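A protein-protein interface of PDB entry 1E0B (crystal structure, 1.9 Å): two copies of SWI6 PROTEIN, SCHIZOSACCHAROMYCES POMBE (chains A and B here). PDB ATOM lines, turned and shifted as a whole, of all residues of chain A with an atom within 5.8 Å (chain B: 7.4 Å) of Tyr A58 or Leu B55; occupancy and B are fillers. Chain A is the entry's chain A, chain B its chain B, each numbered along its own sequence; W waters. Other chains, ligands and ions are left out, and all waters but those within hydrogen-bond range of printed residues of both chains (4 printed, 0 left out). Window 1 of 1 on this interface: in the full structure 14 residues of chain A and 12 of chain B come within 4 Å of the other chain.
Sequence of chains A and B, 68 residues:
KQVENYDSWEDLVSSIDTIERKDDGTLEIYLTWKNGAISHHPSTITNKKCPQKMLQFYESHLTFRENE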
ATOM      1  N   ILE A  19     -24.203   6.442  31.570  1.00  0.00           N
ATOM      2  CA  ILE A  19     -23.136   6.224  30.604  1.00  0.00           C
ATOM      3  C   ILE A  19     -22.546   7.566  30.192  1.00  0.00           C
ATOM      4  O   ILE A  19     -23.269   8.557  30.098  1.00  0.00           O
ATOM      5  CB  ILE A  19     -23.656   5.507  29.340  1.00  0.00           C
ATOM      6  CG1 ILE A  19     -24.300   4.181  29.733  1.00  0.00           C
ATOM      7  CG2 ILE A  19     -22.507   5.254  28.368  1.00  0.00           C
ATOM      8  CD1 ILE A  19     -24.742   3.344  28.561  1.00  0.00           C
ATOM      9  N   LEU A  27     -16.710   4.687  25.796  1.00  0.00           N
ATOM     10  CA  LEU A  27     -17.830   4.844  26.714  1.00  0.00           C
ATOM     11  C   LEU A  27     -17.451   4.282  28.088  1.00  0.00           C
ATOM     12  O   LEU A  27     -16.847   3.219  28.175  1.00  0.00           O
ATOM     13  CB  LEU A  27     -19.062   4.115  26.163  1.00  0.00           C
ATOM     14  CG  LEU A  27     -19.600   4.656  24.829  1.00  0.00           C
ATOM     15  CD1 LEU A  27     -20.692   3.750  24.288  1.00  0.00           C
ATOM     16  CD2 LEU A  27     -20.147   6.075  25.039  1.00  0.00           C
ATOM     17  N   ILE A  29     -19.004   3.117  31.764  1.00  0.00           N
ATOM     18  CA  ILE A  29     -20.257   2.699  32.390  1.00  0.00           C
ATOM     19  C   ILE A  29     -20.232   2.783  33.916  1.00  0.00           C
ATOM     20  O   ILE A  29     -19.358   2.208  34.559  1.00  0.00           O
ATOM     21  CB  ILE A  29     -20.609   1.234  32.012  1.00  0.00           C
ATOM     22  CG1 ILE A  29     -20.590   1.051  30.486  1.00  0.00           C
ATOM     23  CG2 ILE A  29     -21.952   0.845  32.626  1.00  0.00           C
ATOM     24  CD1 ILE A  29     -21.605   1.878  29.723  1.00  0.00           C
ATOM     25  N   SER A  43     -17.083   0.132  28.462  1.00  0.00           N
ATOM     26  CA  SER A  43     -18.185  -0.639  27.885  1.00  0.00           C
ATOM     27  C   SER A  43     -17.676  -1.905  27.204  1.00  0.00           C
ATOM     28  O   SER A  43     -18.418  -2.875  27.050  1.00  0.00           O
ATOM     29  CB  SER A  43     -19.004   0.215  26.895  1.00  0.00           C
ATOM     30  OG  SER A  43     -18.229   0.652  25.788  1.00  0.00           O
ATOM     31  N   ASN A  47     -19.904  -5.072  28.360  1.00  0.00           N
ATOM     32  CA  ASN A  47     -20.662  -5.779  27.310  1.00  0.00           C
ATOM     33  C   ASN A  47     -20.413  -7.287  27.349  1.00  0.00           C
ATOM     34  O   ASN A  47     -21.306  -8.081  27.033  1.00  0.00           O
ATOM     35  CB  ASN A  47     -20.301  -5.271  25.906  1.00  0.00           C
ATOM     36  CG  ASN A  47     -20.852  -3.884  25.617  1.00  0.00           C
ATOM     37  OD1 ASN A  47     -21.755  -3.392  26.302  1.00  0.00           O
ATOM     38  ND2 ASN A  47     -20.313  -3.251  24.581  1.00  0.00           N
ATOM     39  N   LYS A  48     -19.188  -7.682  27.711  1.00  0.00           N
ATOM     40  CA  LYS A  48     -18.833  -9.109  27.771  1.00  0.00           C
ATOM     41  C   LYS A  48     -19.118  -9.815  29.100  1.00  0.00           C
ATOM     42  O   LYS A  48     -19.446 -11.009  29.097  1.00  0.00           O
ATOM     43  CB  LYS A  48     -17.341  -9.305  27.432  1.00  0.00           C
ATOM     44  CG  LYS A  48     -16.943  -8.974  25.993  1.00  0.00           C
ATOM     45  CD  LYS A  48     -17.747  -9.799  24.996  1.00  0.00           C
ATOM     46  CE  LYS A  48     -17.210  -9.623  23.596  1.00  0.00           C
ATOM     47  NZ  LYS A  48     -17.068  -8.188  23.243  1.00  0.00           N
ATOM     48  N   PRO A  51     -23.707  -8.795  29.446  1.00  0.00           N
ATOM     49  CA  PRO A  51     -24.440  -8.292  28.277  1.00  0.00           C
ATOM     50  C   PRO A  51     -25.956  -8.143  28.439  1.00  0.00           C
ATOM     51  O   PRO A  51     -26.523  -7.178  27.927  1.00  0.00           O
ATOM     52  CB  PRO A  51     -24.031  -9.253  27.159  1.00  0.00           C
ATOM     53  CG  PRO A  51     -23.839 -10.578  27.879  1.00  0.00           C
ATOM     54  CD  PRO A  51     -23.150 -10.143  29.203  1.00  0.00           C
ATOM     55  N   LYS A  53     -27.591  -7.378  31.166  1.00  0.00           N
ATOM     56  CA  LYS A  53     -27.830  -6.189  32.008  1.00  0.00           C
ATOM     57  C   LYS A  53     -27.706  -4.943  31.123  1.00  0.00           C
ATOM     58  O   LYS A  53     -28.507  -3.997  31.223  1.00  0.00           O
ATOM     59  CB  LYS A  53     -26.815  -6.094  33.167  1.00  0.00           C
ATOM     60  CG  LYS A  53     -27.106  -7.010  34.331  1.00  0.00           C
ATOM     61  CD  LYS A  53     -28.406  -6.620  35.002  1.00  0.00           C
ATOM     62  CE  LYS A  53     -28.629  -7.410  36.275  1.00  0.00           C
ATOM     63  NZ  LYS A  53     -29.763  -6.840  37.063  1.00  0.00           N
ATOM     64  N   MET A  54     -26.710  -4.945  30.240  1.00  0.00           N
ATOM     65  CA  MET A  54     -26.508  -3.811  29.328  1.00  0.00           C
ATOM     66  C   MET A  54     -27.688  -3.624  28.350  1.00  0.00           C
ATOM     67  O   MET A  54     -28.089  -2.498  28.069  1.00  0.00           O
ATOM     68  CB  MET A  54     -25.213  -3.985  28.509  1.00  0.00           C
ATOM     69  CG  MET A  54     -23.911  -3.905  29.318  1.00  0.00           C
ATOM     70  SD  MET A  54     -23.689  -2.353  30.242  1.00  0.00           S
ATOM     71  CE  MET A  54     -23.494  -1.159  28.970  1.00  0.00           C
ATOM     72  N   LEU A  55     -28.224  -4.725  27.835  1.00  0.00           N
ATOM     73  CA  LEU A  55     -29.337  -4.661  26.882  1.00  0.00           C
ATOM     74  C   LEU A  55     -30.629  -4.124  27.521  1.00  0.00           C
ATOM     75  O   LEU A  55     -31.378  -3.368  26.887  1.00  0.00           O
ATOM     76  CB  LEU A  55     -29.565  -6.039  26.270  1.00  0.00           C
ATOM     77  CG  LEU A  55     -28.467  -6.493  25.277  1.00  0.00           C
ATOM     78  CD1 LEU A  55     -28.638  -7.974  25.003  1.00  0.00           C
ATOM     79  CD2 LEU A  55     -28.536  -5.692  23.963  1.00  0.00           C
ATOM     80  N   GLN A  56     -30.899  -4.524  28.760  1.00  0.00           N
ATOM     81  CA  GLN A  56     -32.082  -4.032  29.465  1.00  0.00           C
ATOM     82  C   GLN A  56     -31.985  -2.518  29.628  1.00  0.00           C
ATOM     83  O   GLN A  56     -32.978  -1.799  29.492  1.00  0.00           O
ATOM     84  CB  GLN A  56     -32.193  -4.668  30.848  1.00  0.00           C
ATOM     85  CG  GLN A  56     -32.490  -6.136  30.822  1.00  0.00           C
ATOM     86  CD  GLN A  56     -32.512  -6.740  32.212  1.00  0.00           C
ATOM     87  OE1 GLN A  56     -32.942  -7.883  32.393  1.00  0.00           O
ATOM     88  NE2 GLN A  56     -32.040  -5.980  33.205  1.00  0.00           N
ATOM     89  N   PHE A  57     -30.787  -2.037  29.938  1.00  0.00           N
ATOM     90  CA  PHE A  57     -30.560  -0.600  30.097  1.00  0.00           C
ATOM     91  C   PHE A  57     -30.868   0.160  28.804  1.00  0.00           C
ATOM     92  O   PHE A  57     -31.523   1.209  28.820  1.00  0.00           O
ATOM     93  CB  PHE A  57     -29.105  -0.328  30.488  1.00  0.00           C
ATOM     94  CG  PHE A  57     -28.759   1.133  30.570  1.00  0.00           C
ATOM     95  CD1 PHE A  57     -29.059   1.875  31.711  1.00  0.00           C
ATOM     96  CD2 PHE A  57     -28.127   1.773  29.506  1.00  0.00           C
ATOM     97  CE1 PHE A  57     -28.733   3.229  31.792  1.00  0.00           C
ATOM     98  CE2 PHE A  57     -27.798   3.125  29.576  1.00  0.00           C
ATOM     99  CZ  PHE A  57     -28.101   3.855  30.721  1.00  0.00           C
ATOM    100  N   TYR A  58     -30.382  -0.351  27.680  1.00  0.00           N
ATOM    101  CA  TYR A  58     -30.613   0.323  26.403  1.00  0.00           C
ATOM    102  C   TYR A  58     -32.084   0.359  25.980  1.00  0.00           C
ATOM    103  O   TYR A  58     -32.547   1.358  25.417  1.00  0.00           O
ATOM    104  CB  TYR A  58     -29.749  -0.327  25.311  1.00  0.00           C
ATOM    105  CG  TYR A  58     -28.279   0.059  25.414  1.00  0.00           C
ATOM    106  CD1 TYR A  58     -27.894   1.401  25.478  1.00  0.00           C
ATOM    107  CD2 TYR A  58     -27.276  -0.913  25.440  1.00  0.00           C
ATOM    108  CE1 TYR A  58     -26.546   1.768  25.564  1.00  0.00           C
ATOM    109  CE2 TYR A  58     -25.922  -0.557  25.524  1.00  0.00           C
ATOM    110  CZ  TYR A  58     -25.567   0.777  25.584  1.00  0.00           C
ATOM    111  OH  TYR A  58     -24.232   1.122  25.638  1.00  0.00           O
ATOM    112  N   GLU A  59     -32.811  -0.707  26.250  1.00  0.00           N
ATOM    113  CA  GLU A  59     -34.222  -0.733  25.876  1.00  0.00           C
ATOM    114  C   GLU A  59     -35.040   0.267  26.689  1.00  0.00           C
ATOM    115  O   GLU A  59     -36.068   0.764  26.220  1.00  0.00           O
ATOM    116  CB  GLU A  59     -34.813  -2.130  26.050  1.00  0.00           C
ATOM    117  CG  GLU A  59     -34.162  -3.173  25.165  1.00  0.00           C
ATOM    118  CD  GLU A  59     -34.977  -4.439  25.056  1.00  0.00           C
ATOM    119  OE1 GLU A  59     -35.813  -4.695  25.947  1.00  0.00           O
ATOM    120  OE2 GLU A  59     -34.771  -5.187  24.079  1.00  0.00           O
ATOM    121  N   SER A  60     -34.701   0.575  27.920  1.00  0.00           N
ATOM    122  CA  SER A  60     -35.510   1.473  28.802  1.00  0.00           C
ATOM    123  C   SER A  60     -34.988   2.910  28.691  1.00  0.00           C
ATOM    124  O   SER A  60     -34.768   3.619  29.668  1.00  0.00           O
ATOM    125  CB  SER A  60     -35.276   1.113  30.264  1.00  0.00           C
ATOM    126  OG  SER A  60     -34.053   1.655  30.733  1.00  0.00           O
ATOM    127  N   HIS A  61     -34.758   3.238  27.430  1.00  0.00           N
ATOM    128  CA  HIS A  61     -33.877   4.296  27.034  1.00  0.00           C
ATOM    129  C   HIS A  61     -33.683   4.216  25.538  1.00  0.00           C
ATOM    130  O   HIS A  61     -32.624   3.895  24.992  1.00  0.00           O
ATOM    131  CB  HIS A  61     -32.584   3.980  27.680  1.00  0.00           C
ATOM    132  CG  HIS A  61     -31.983   5.050  28.563  1.00  0.00           C
ATOM    133  ND1 HIS A  61     -32.282   5.282  29.881  1.00  0.00           N
ATOM    134  CD2 HIS A  61     -31.054   5.963  28.197  1.00  0.00           C
ATOM    135  CE1 HIS A  61     -31.550   6.299  30.301  1.00  0.00           C
ATOM    136  NE2 HIS A  61     -30.784   6.733  29.304  1.00  0.00           N
ATOM    137  N   LEU A  62     -34.825   4.477  24.983  1.00  0.00           N
ATOM    138  CA  LEU A  62     -35.125   4.331  23.608  1.00  0.00           C
ATOM    139  C   LEU A  62     -36.184   5.349  23.160  1.00  0.00           C
ATOM    140  O   LEU A  62     -36.188   5.791  22.011  1.00  0.00           O
ATOM    141  CB  LEU A  62     -35.641   2.906  23.421  1.00  0.00           C
ATOM    142  CG  LEU A  62     -35.323   2.135  22.137  1.00  0.00           C
ATOM    143  CD1 LEU A  62     -33.869   1.696  22.080  1.00  0.00           C
ATOM    144  CD2 LEU A  62     -36.251   0.945  22.008  1.00  0.00           C
ATOM    145  N   ILE B  16     -27.083  -5.270  12.506  1.00  0.00           N
ATOM    146  CA  ILE B  16     -28.437  -4.908  12.975  1.00  0.00           C
ATOM    147  C   ILE B  16     -28.631  -3.546  12.289  1.00  0.00           C
ATOM    148  O   ILE B  16     -27.748  -2.680  12.376  1.00  0.00           O
ATOM    149  CB  ILE B  16     -28.480  -4.752  14.522  1.00  0.00           C
ATOM    150  CG1 ILE B  16     -28.054  -6.059  15.194  1.00  0.00           C
ATOM    151  CG2 ILE B  16     -29.885  -4.357  14.985  1.00  0.00           C
ATOM    152  CD1 ILE B  16     -29.025  -7.267  15.031  1.00  0.00           C
ATOM    153  N   ARG B  21     -40.653   0.215  17.505  1.00  0.00           N
ATOM    154  CA  ARG B  21     -41.411  -0.037  18.723  1.00  0.00           C
ATOM    155  C   ARG B  21     -42.883  -0.283  18.370  1.00  0.00           C
ATOM    156  O   ARG B  21     -43.646   0.657  18.175  1.00  0.00           O
ATOM    157  CB  ARG B  21     -41.282   1.163  19.665  1.00  0.00           C
ATOM    158  CG  ARG B  21     -42.129   1.078  20.920  1.00  0.00           C
ATOM    159  CD  ARG B  21     -41.280   1.302  22.153  1.00  0.00           C
ATOM    160  NE  ARG B  21     -40.899   0.041  22.785  1.00  0.00           N
ATOM    161  CZ  ARG B  21     -40.011  -0.062  23.767  1.00  0.00           C
ATOM    162  NH1 ARG B  21     -39.406   1.025  24.229  1.00  0.00           N
ATOM    163  NH2 ARG B  21     -39.735  -1.248  24.299  1.00  0.00           N
ATOM    164  N   LEU B  27     -40.521  -4.729  20.643  1.00  0.00           N
ATOM    165  CA  LEU B  27     -39.533  -4.202  19.704  1.00  0.00           C
ATOM    166  C   LEU B  27     -39.308  -5.187  18.562  1.00  0.00           C
ATOM    167  O   LEU B  27     -39.148  -6.379  18.785  1.00  0.00           O
ATOM    168  CB  LEU B  27     -38.199  -3.943  20.420  1.00  0.00           C
ATOM    169  CG  LEU B  27     -38.188  -2.836  21.475  1.00  0.00           C
ATOM    170  CD1 LEU B  27     -36.880  -2.870  22.244  1.00  0.00           C
ATOM    171  CD2 LEU B  27     -38.382  -1.479  20.807  1.00  0.00           C
ATOM    172  N   ASN B  47     -31.816 -10.688  21.302  1.00  0.00           N
ATOM    173  CA  ASN B  47     -31.072 -10.427  22.547  1.00  0.00           C
ATOM    174  C   ASN B  47     -30.324 -11.677  23.029  1.00  0.00           C
ATOM    175  O   ASN B  47     -29.230 -11.577  23.597  1.00  0.00           O
ATOM    176  CB  ASN B  47     -32.002  -9.950  23.670  1.00  0.00           C
ATOM    177  CG  ASN B  47     -32.340  -8.472  23.577  1.00  0.00           C
ATOM    178  OD1 ASN B  47     -31.744  -7.720  22.797  1.00  0.00           O
ATOM    179  ND2 ASN B  47     -33.296  -8.040  24.394  1.00  0.00           N
ATOM    180  N   CYS B  50     -27.834 -13.172  19.412  1.00  0.00           N
ATOM    181  CA  CYS B  50     -26.696 -12.348  19.004  1.00  0.00           C
ATOM    182  C   CYS B  50     -26.569 -11.051  19.824  1.00  0.00           C
ATOM    183  O   CYS B  50     -26.601  -9.936  19.294  1.00  0.00           O
ATOM    184  CB  CYS B  50     -26.757 -12.048  17.493  1.00  0.00           C
ATOM    185  SG  CYS B  50     -28.355 -11.403  16.805  1.00  0.00           S
ATOM    186  N   PRO B  51     -26.383 -11.188  21.149  1.00  0.00           N
ATOM    187  CA  PRO B  51     -26.254 -10.016  22.027  1.00  0.00           C
ATOM    188  C   PRO B  51     -25.167  -9.000  21.686  1.00  0.00           C
ATOM    189  O   PRO B  51     -25.382  -7.796  21.834  1.00  0.00           O
ATOM    190  CB  PRO B  51     -26.073 -10.633  23.425  1.00  0.00           C
ATOM    191  CG  PRO B  51     -25.583 -12.033  23.169  1.00  0.00           C
ATOM    192  CD  PRO B  51     -26.354 -12.441  21.927  1.00  0.00           C
ATOM    193  N   GLN B  52     -24.001  -9.464  21.232  1.00  0.00           N
ATOM    194  CA  GLN B  52     -22.935  -8.539  20.911  1.00  0.00           C
ATOM    195  C   GLN B  52     -23.272  -7.713  19.665  1.00  0.00           C
ATOM    196  O   GLN B  52     -22.899  -6.537  19.565  1.00  0.00           O
ATOM    197  CB  GLN B  52     -21.603  -9.303  20.749  1.00  0.00           C
ATOM    198  CG  GLN B  52     -21.124  -9.993  22.023  1.00  0.00           C
ATOM    199  CD  GLN B  52     -21.038  -9.054  23.216  1.00  0.00           C
ATOM    200  OE1 GLN B  52     -20.615  -7.904  23.092  1.00  0.00           O
ATOM    201  NE2 GLN B  52     -21.426  -9.547  24.379  1.00  0.00           N
ATOM    202  N   LYS B  53     -23.953  -8.304  18.698  1.00  0.00           N
ATOM    203  CA  LYS B  53     -24.346  -7.510  17.512  1.00  0.00           C
ATOM    204  C   LYS B  53     -25.379  -6.424  17.954  1.00  0.00           C
ATOM    205  O   LYS B  53     -25.361  -5.286  17.454  1.00  0.00           O
ATOM    206  CB  LYS B  53     -24.982  -8.411  16.448  1.00  0.00           C
ATOM    207  CG  LYS B  53     -24.044  -9.455  15.836  1.00  0.00           C
ATOM    208  CD  LYS B  53     -23.056  -8.813  14.900  1.00  0.00           C
ATOM    209  CE  LYS B  53     -22.077  -9.850  14.352  1.00  0.00           C
ATOM    210  NZ  LYS B  53     -21.185  -9.189  13.364  1.00  0.00           N
ATOM    211  N   MET B  54     -26.277  -6.781  18.874  1.00  0.00           N
ATOM    212  CA  MET B  54     -27.279  -5.821  19.374  1.00  0.00           C
ATOM    213  C   MET B  54     -26.575  -4.653  20.081  1.00  0.00           C
ATOM    214  O   MET B  54     -26.894  -3.481  19.842  1.00  0.00           O
ATOM    215  CB  MET B  54     -28.244  -6.493  20.358  1.00  0.00           C
ATOM    216  CG  MET B  54     -29.263  -7.463  19.760  1.00  0.00           C
ATOM    217  SD  MET B  54     -30.295  -6.723  18.429  1.00  0.00           S
ATOM    218  CE  MET B  54     -31.282  -5.603  19.401  1.00  0.00           C
ATOM    219  N   LEU B  55     -25.617  -4.969  20.960  1.00  0.00           N
ATOM    220  CA  LEU B  55     -24.887  -3.923  21.684  1.00  0.00           C
ATOM    221  C   LEU B  55     -24.114  -2.979  20.757  1.00  0.00           C
ATOM    222  O   LEU B  55     -23.991  -1.784  21.034  1.00  0.00           O
ATOM    223  CB  LEU B  55     -23.950  -4.560  22.729  1.00  0.00           C
ATOM    224  CG  LEU B  55     -24.706  -5.210  23.912  1.00  0.00           C
ATOM    225  CD1 LEU B  55     -23.754  -6.085  24.762  1.00  0.00           C
ATOM    226  CD2 LEU B  55     -25.335  -4.116  24.780  1.00  0.00           C
ATOM    227  N   GLN B  56     -23.578  -3.499  19.661  1.00  0.00           N
ATOM    228  CA  GLN B  56     -22.874  -2.637  18.695  1.00  0.00           C
ATOM    229  C   GLN B  56     -23.833  -1.593  18.066  1.00  0.00           C
ATOM    230  O   GLN B  56     -23.449  -0.439  17.824  1.00  0.00           O
ATOM    231  CB  GLN B  56     -22.256  -3.485  17.576  1.00  0.00           C
ATOM    232  CG  GLN B  56     -21.088  -4.329  18.030  1.00  0.00           C
ATOM    233  CD  GLN B  56     -19.983  -3.472  18.613  1.00  0.00           C
ATOM    234  OE1 GLN B  56     -19.432  -2.615  17.923  1.00  0.00           O
ATOM    235  NE2 GLN B  56     -19.654  -3.691  19.891  1.00  0.00           N
ATOM    236  N   PHE B  57     -25.063  -2.012  17.791  1.00  0.00           N
ATOM    237  CA  PHE B  57     -26.075  -1.120  17.200  1.00  0.00           C
ATOM    238  C   PHE B  57     -26.437  -0.004  18.181  1.00  0.00           C
ATOM    239  O   PHE B  57     -26.430   1.179  17.821  1.00  0.00           O
ATOM    240  CB  PHE B  57     -27.335  -1.920  16.824  1.00  0.00           C
ATOM    241  CG  PHE B  57     -28.494  -1.059  16.345  1.00  0.00           C
ATOM    242  CD1 PHE B  57     -28.537  -0.589  15.033  1.00  0.00           C
ATOM    243  CD2 PHE B  57     -29.525  -0.709  17.216  1.00  0.00           C
ATOM    244  CE1 PHE B  57     -29.599   0.219  14.587  1.00  0.00           C
ATOM    245  CE2 PHE B  57     -30.596   0.102  16.787  1.00  0.00           C
ATOM    246  CZ  PHE B  57     -30.625   0.561  15.472  1.00  0.00           C
ATOM    247  N   TYR B  58     -26.754  -0.373  19.419  1.00  0.00           N
ATOM    248  CA  TYR B  58     -27.096   0.614  20.439  1.00  0.00           C
ATOM    249  C   TYR B  58     -25.973   1.627  20.649  1.00  0.00           C
ATOM    250  O   TYR B  58     -26.244   2.832  20.762  1.00  0.00           O
ATOM    251  CB  TYR B  58     -27.453  -0.091  21.756  1.00  0.00           C
ATOM    252  CG  TYR B  58     -28.813  -0.763  21.736  1.00  0.00           C
ATOM    253  CD1 TYR B  58     -29.944  -0.086  21.273  1.00  0.00           C
ATOM    254  CD2 TYR B  58     -28.968  -2.080  22.167  1.00  0.00           C
ATOM    255  CE1 TYR B  58     -31.197  -0.712  21.236  1.00  0.00           C
ATOM    256  CE2 TYR B  58     -30.212  -2.716  22.138  1.00  0.00           C
ATOM    257  CZ  TYR B  58     -31.327  -2.019  21.664  1.00  0.00           C
ATOM    258  OH  TYR B  58     -32.562  -2.641  21.595  1.00  0.00           O
ATOM    259  N   GLU B  59     -24.715   1.175  20.677  1.00  0.00           N
ATOM    260  CA  GLU B  59     -23.597   2.118  20.875  1.00  0.00           C
ATOM    261  C   GLU B  59     -23.449   3.110  19.717  1.00  0.00           C
ATOM    262  O   GLU B  59     -23.058   4.252  19.930  1.00  0.00           O
ATOM    263  CB  GLU B  59     -22.254   1.384  21.081  1.00  0.00           C
ATOM    264  CG  GLU B  59     -22.133   0.668  22.423  1.00  0.00           C
ATOM    265  CD  GLU B  59     -20.710   0.205  22.759  1.00  0.00           C
ATOM    266  OE1 GLU B  59     -19.842   0.173  21.862  1.00  0.00           O
ATOM    267  OE2 GLU B  59     -20.466  -0.145  23.934  1.00  0.00           O
ATOM    268  N   SER B  60     -23.745   2.672  18.499  1.00  0.00           N
ATOM    269  CA  SER B  60     -23.640   3.555  17.339  1.00  0.00           C
ATOM    270  C   SER B  60     -24.865   4.467  17.273  1.00  0.00           C
ATOM    271  O   SER B  60     -24.861   5.500  16.599  1.00  0.00           O
ATOM    272  CB  SER B  60     -23.562   2.727  16.062  1.00  0.00           C
ATOM    273  OG  SER B  60     -24.764   1.999  15.879  1.00  0.00           O
ATOM    274  N   HIS B  61     -25.914   4.065  17.978  1.00  0.00           N
ATOM    275  CA  HIS B  61     -27.165   4.812  18.021  1.00  0.00           C
ATOM    276  C   HIS B  61     -27.237   5.669  19.276  1.00  0.00           C
ATOM    277  O   HIS B  61     -28.322   5.963  19.777  1.00  0.00           O
ATOM    278  CB  HIS B  61     -28.341   3.839  18.010  1.00  0.00           C
ATOM    279  CG  HIS B  61     -29.310   4.082  16.901  1.00  0.00           C
ATOM    280  ND1 HIS B  61     -28.929   4.108  15.576  1.00  0.00           N
ATOM    281  CD2 HIS B  61     -30.643   4.320  16.915  1.00  0.00           C
ATOM    282  CE1 HIS B  61     -29.986   4.354  14.822  1.00  0.00           C
ATOM    283  NE2 HIS B  61     -31.040   4.487  15.610  1.00  0.00           N
ATOM    284  N   LEU B  62     -26.075   6.075  19.774  1.00  0.00           N
ATOM    285  CA  LEU B  62     -25.999   6.876  20.987  1.00  0.00           C
ATOM    286  C   LEU B  62     -25.778   8.356  20.701  1.00  0.00           C
ATOM    287  O   LEU B  62     -24.748   8.758  20.157  1.00  0.00           O
ATOM    288  CB  LEU B  62     -24.870   6.349  21.879  1.00  0.00           C
ATOM    289  CG  LEU B  62     -24.874   6.744  23.353  1.00  0.00           C
ATOM    290  CD1 LEU B  62     -26.125   6.197  24.012  1.00  0.00           C
ATOM    291  CD2 LEU B  62     -23.635   6.198  24.034  1.00  0.00           C
HETATM  292  O   HOH W   1     -39.172   0.609  27.135  1.00  0.00           O
HETATM  293  O   HOH W   2     -36.534  -7.276  25.114  1.00  0.00           O
HETATM  294  O   HOH W   3     -32.864  -4.945  22.377  1.00  0.00           O
HETATM  295  O   HOH W   4     -22.332  -0.688  25.604  1.00  0.00           O
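Printed residues of chain B within 4 Å of Asn A47: Gln B52, Leu B55 and Glu B59.
Lys A53 touches none of the printed residues of chain B.
Printed residues of chain B within 4 Å of Leu A55: Asn B47 (3.8 Å), Met B54 (3.7 Å), Leu B55 (3.7 Å) and Tyr B58 (3.9 Å).
Of the printed residues of chain A, Arg B21 touches Glu A59 (3.9 Å) and Leu A62 (3.9 Å).
Lys B53 touches none of the printed residues of chain A.
Of the printed residues of chain A, Leu B55 touches Asn A47 (3.7 Å), Pro A51 (3.98 Å), Met A54 (3.7 Å), Leu A55 (3.7 Å) and Tyr A58 (3.7 Å).
Printed residues of chain A within 4 Å of Leu B62: Leu A27 (3.6 Å).
The nearest residue of chain B that does not touch Tyr A58 is Leu B62 (4.7 Å).
Leu A27 touches Glu B59, and with the chains exchanged Glu A59 touches Leu B27.
Pro A51 touches Leu B55, but with the chains exchanged Leu A55 does not touch Pro B51 (4.02 Å).
Leu A55 touches Tyr B58, and with the chains exchanged Tyr A58 touches Leu B55.
Leu A62 touches Tyr B58, but with the chains exchanged Tyr A58 does not touch Leu B62 (4.7 Å).
Of the 24 pairs that touch across the chains among the printed residues, 16 have their exchanged pair printed and touching as well.
Among the printed residues, merely in contact across the chains: Leu A62 with Leu B27, Lys A48 with Gln B52, Glu A59 with Leu B27, Leu A27 with Leu B62, Leu A55 with Leu B55, Tyr A58 with Leu B55, Tyr A58 with Tyr B58, Asn A47 with Leu B55, Leu A62 with Tyr B58, Leu A55 with Met B54, Met A54 with Leu B55, Leu A55 with Asn B47, Pro A51 with Gln B52, Leu A62 with Arg B21, Leu A27 with Glu B59, Tyr A58 with Glu B59, Leu A55 with Tyr B58, Glu A59 with Arg B21, Glu A59 with Tyr B58 and Pro A51 with Leu B55.
Water W3 lies within hydrogen-bond range of OH of Tyr B58, OE2 of Glu A59 and OD1 of Asn B47.
Water W4 lies within hydrogen-bond range of OE2 of Glu B59 (2.6 Å), OH of Tyr A58 (2.6 Å) and OD1 of Asn A47 (2.9 Å).
Water W2 bridges OE1 of Glu A59 (2.8 Å) and ND2 of Asn B47 (3.4 Å).
Water W1 lies within hydrogen-bond range of NH1 of Arg B21 (2.9 Å) and O of Glu A59 (3.2 Å).
The side-chain carboxylate (OE2) of Glu B59 sits at hydrogen-bond distance from the side-chain hydroxyl (OG) of Ser A43 (3.0 Å).
The backbone carbonyl oxygen of Asn A47 lies within hydrogen-bond range of the side-chain amide nitrogen of Gln B52 (3.0 Å).
ND2 of Asn A47 lies within hydrogen-bond range of OE2 of Glu B59 (3.2 Å).
OE2 of Glu A59 sits at hydrogen-bond distance from ND2 of Asn B47, 3.2 Å away.
Printed residues of chain B that touch a printed residue of chain A: Arg B21, Leu B27, Asn B47, Gln B52, Met B54, Leu B55, Tyr B58, Glu B59 and Leu B62.
Hydrophobic or aromatic side chains of chain B within 4 Å of the printed part of chain A: Leu B27, Met B54, Leu B55, Tyr B58 and Leu B62.
Of the 17 printed residues of chain A, 10 touch a printed residue of chain B.
Hydrophobic or aromatic side chains of chain A within 4 Å of the printed part of chain B: Leu A27, Pro A51, Met A54, Leu A55, Tyr A58 and Leu A62.
Among the printed residues, 24 pairs touch across the chains.
Among the printed residues, no Asp or Glu carboxylate lies within 4 Å of a Lys or Arg side-chain nitrogen of the other chain.
The backbone NH (N) of Ser A43 lies within hydrogen-bond range of the backbone carbonyl oxygen (O) of Leu A27.
The side-chain amide nitrogen (ND2) of Asn A47 lies close to the backbone carbonyl oxygen (O) of Ser A43 (3.1 Å).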
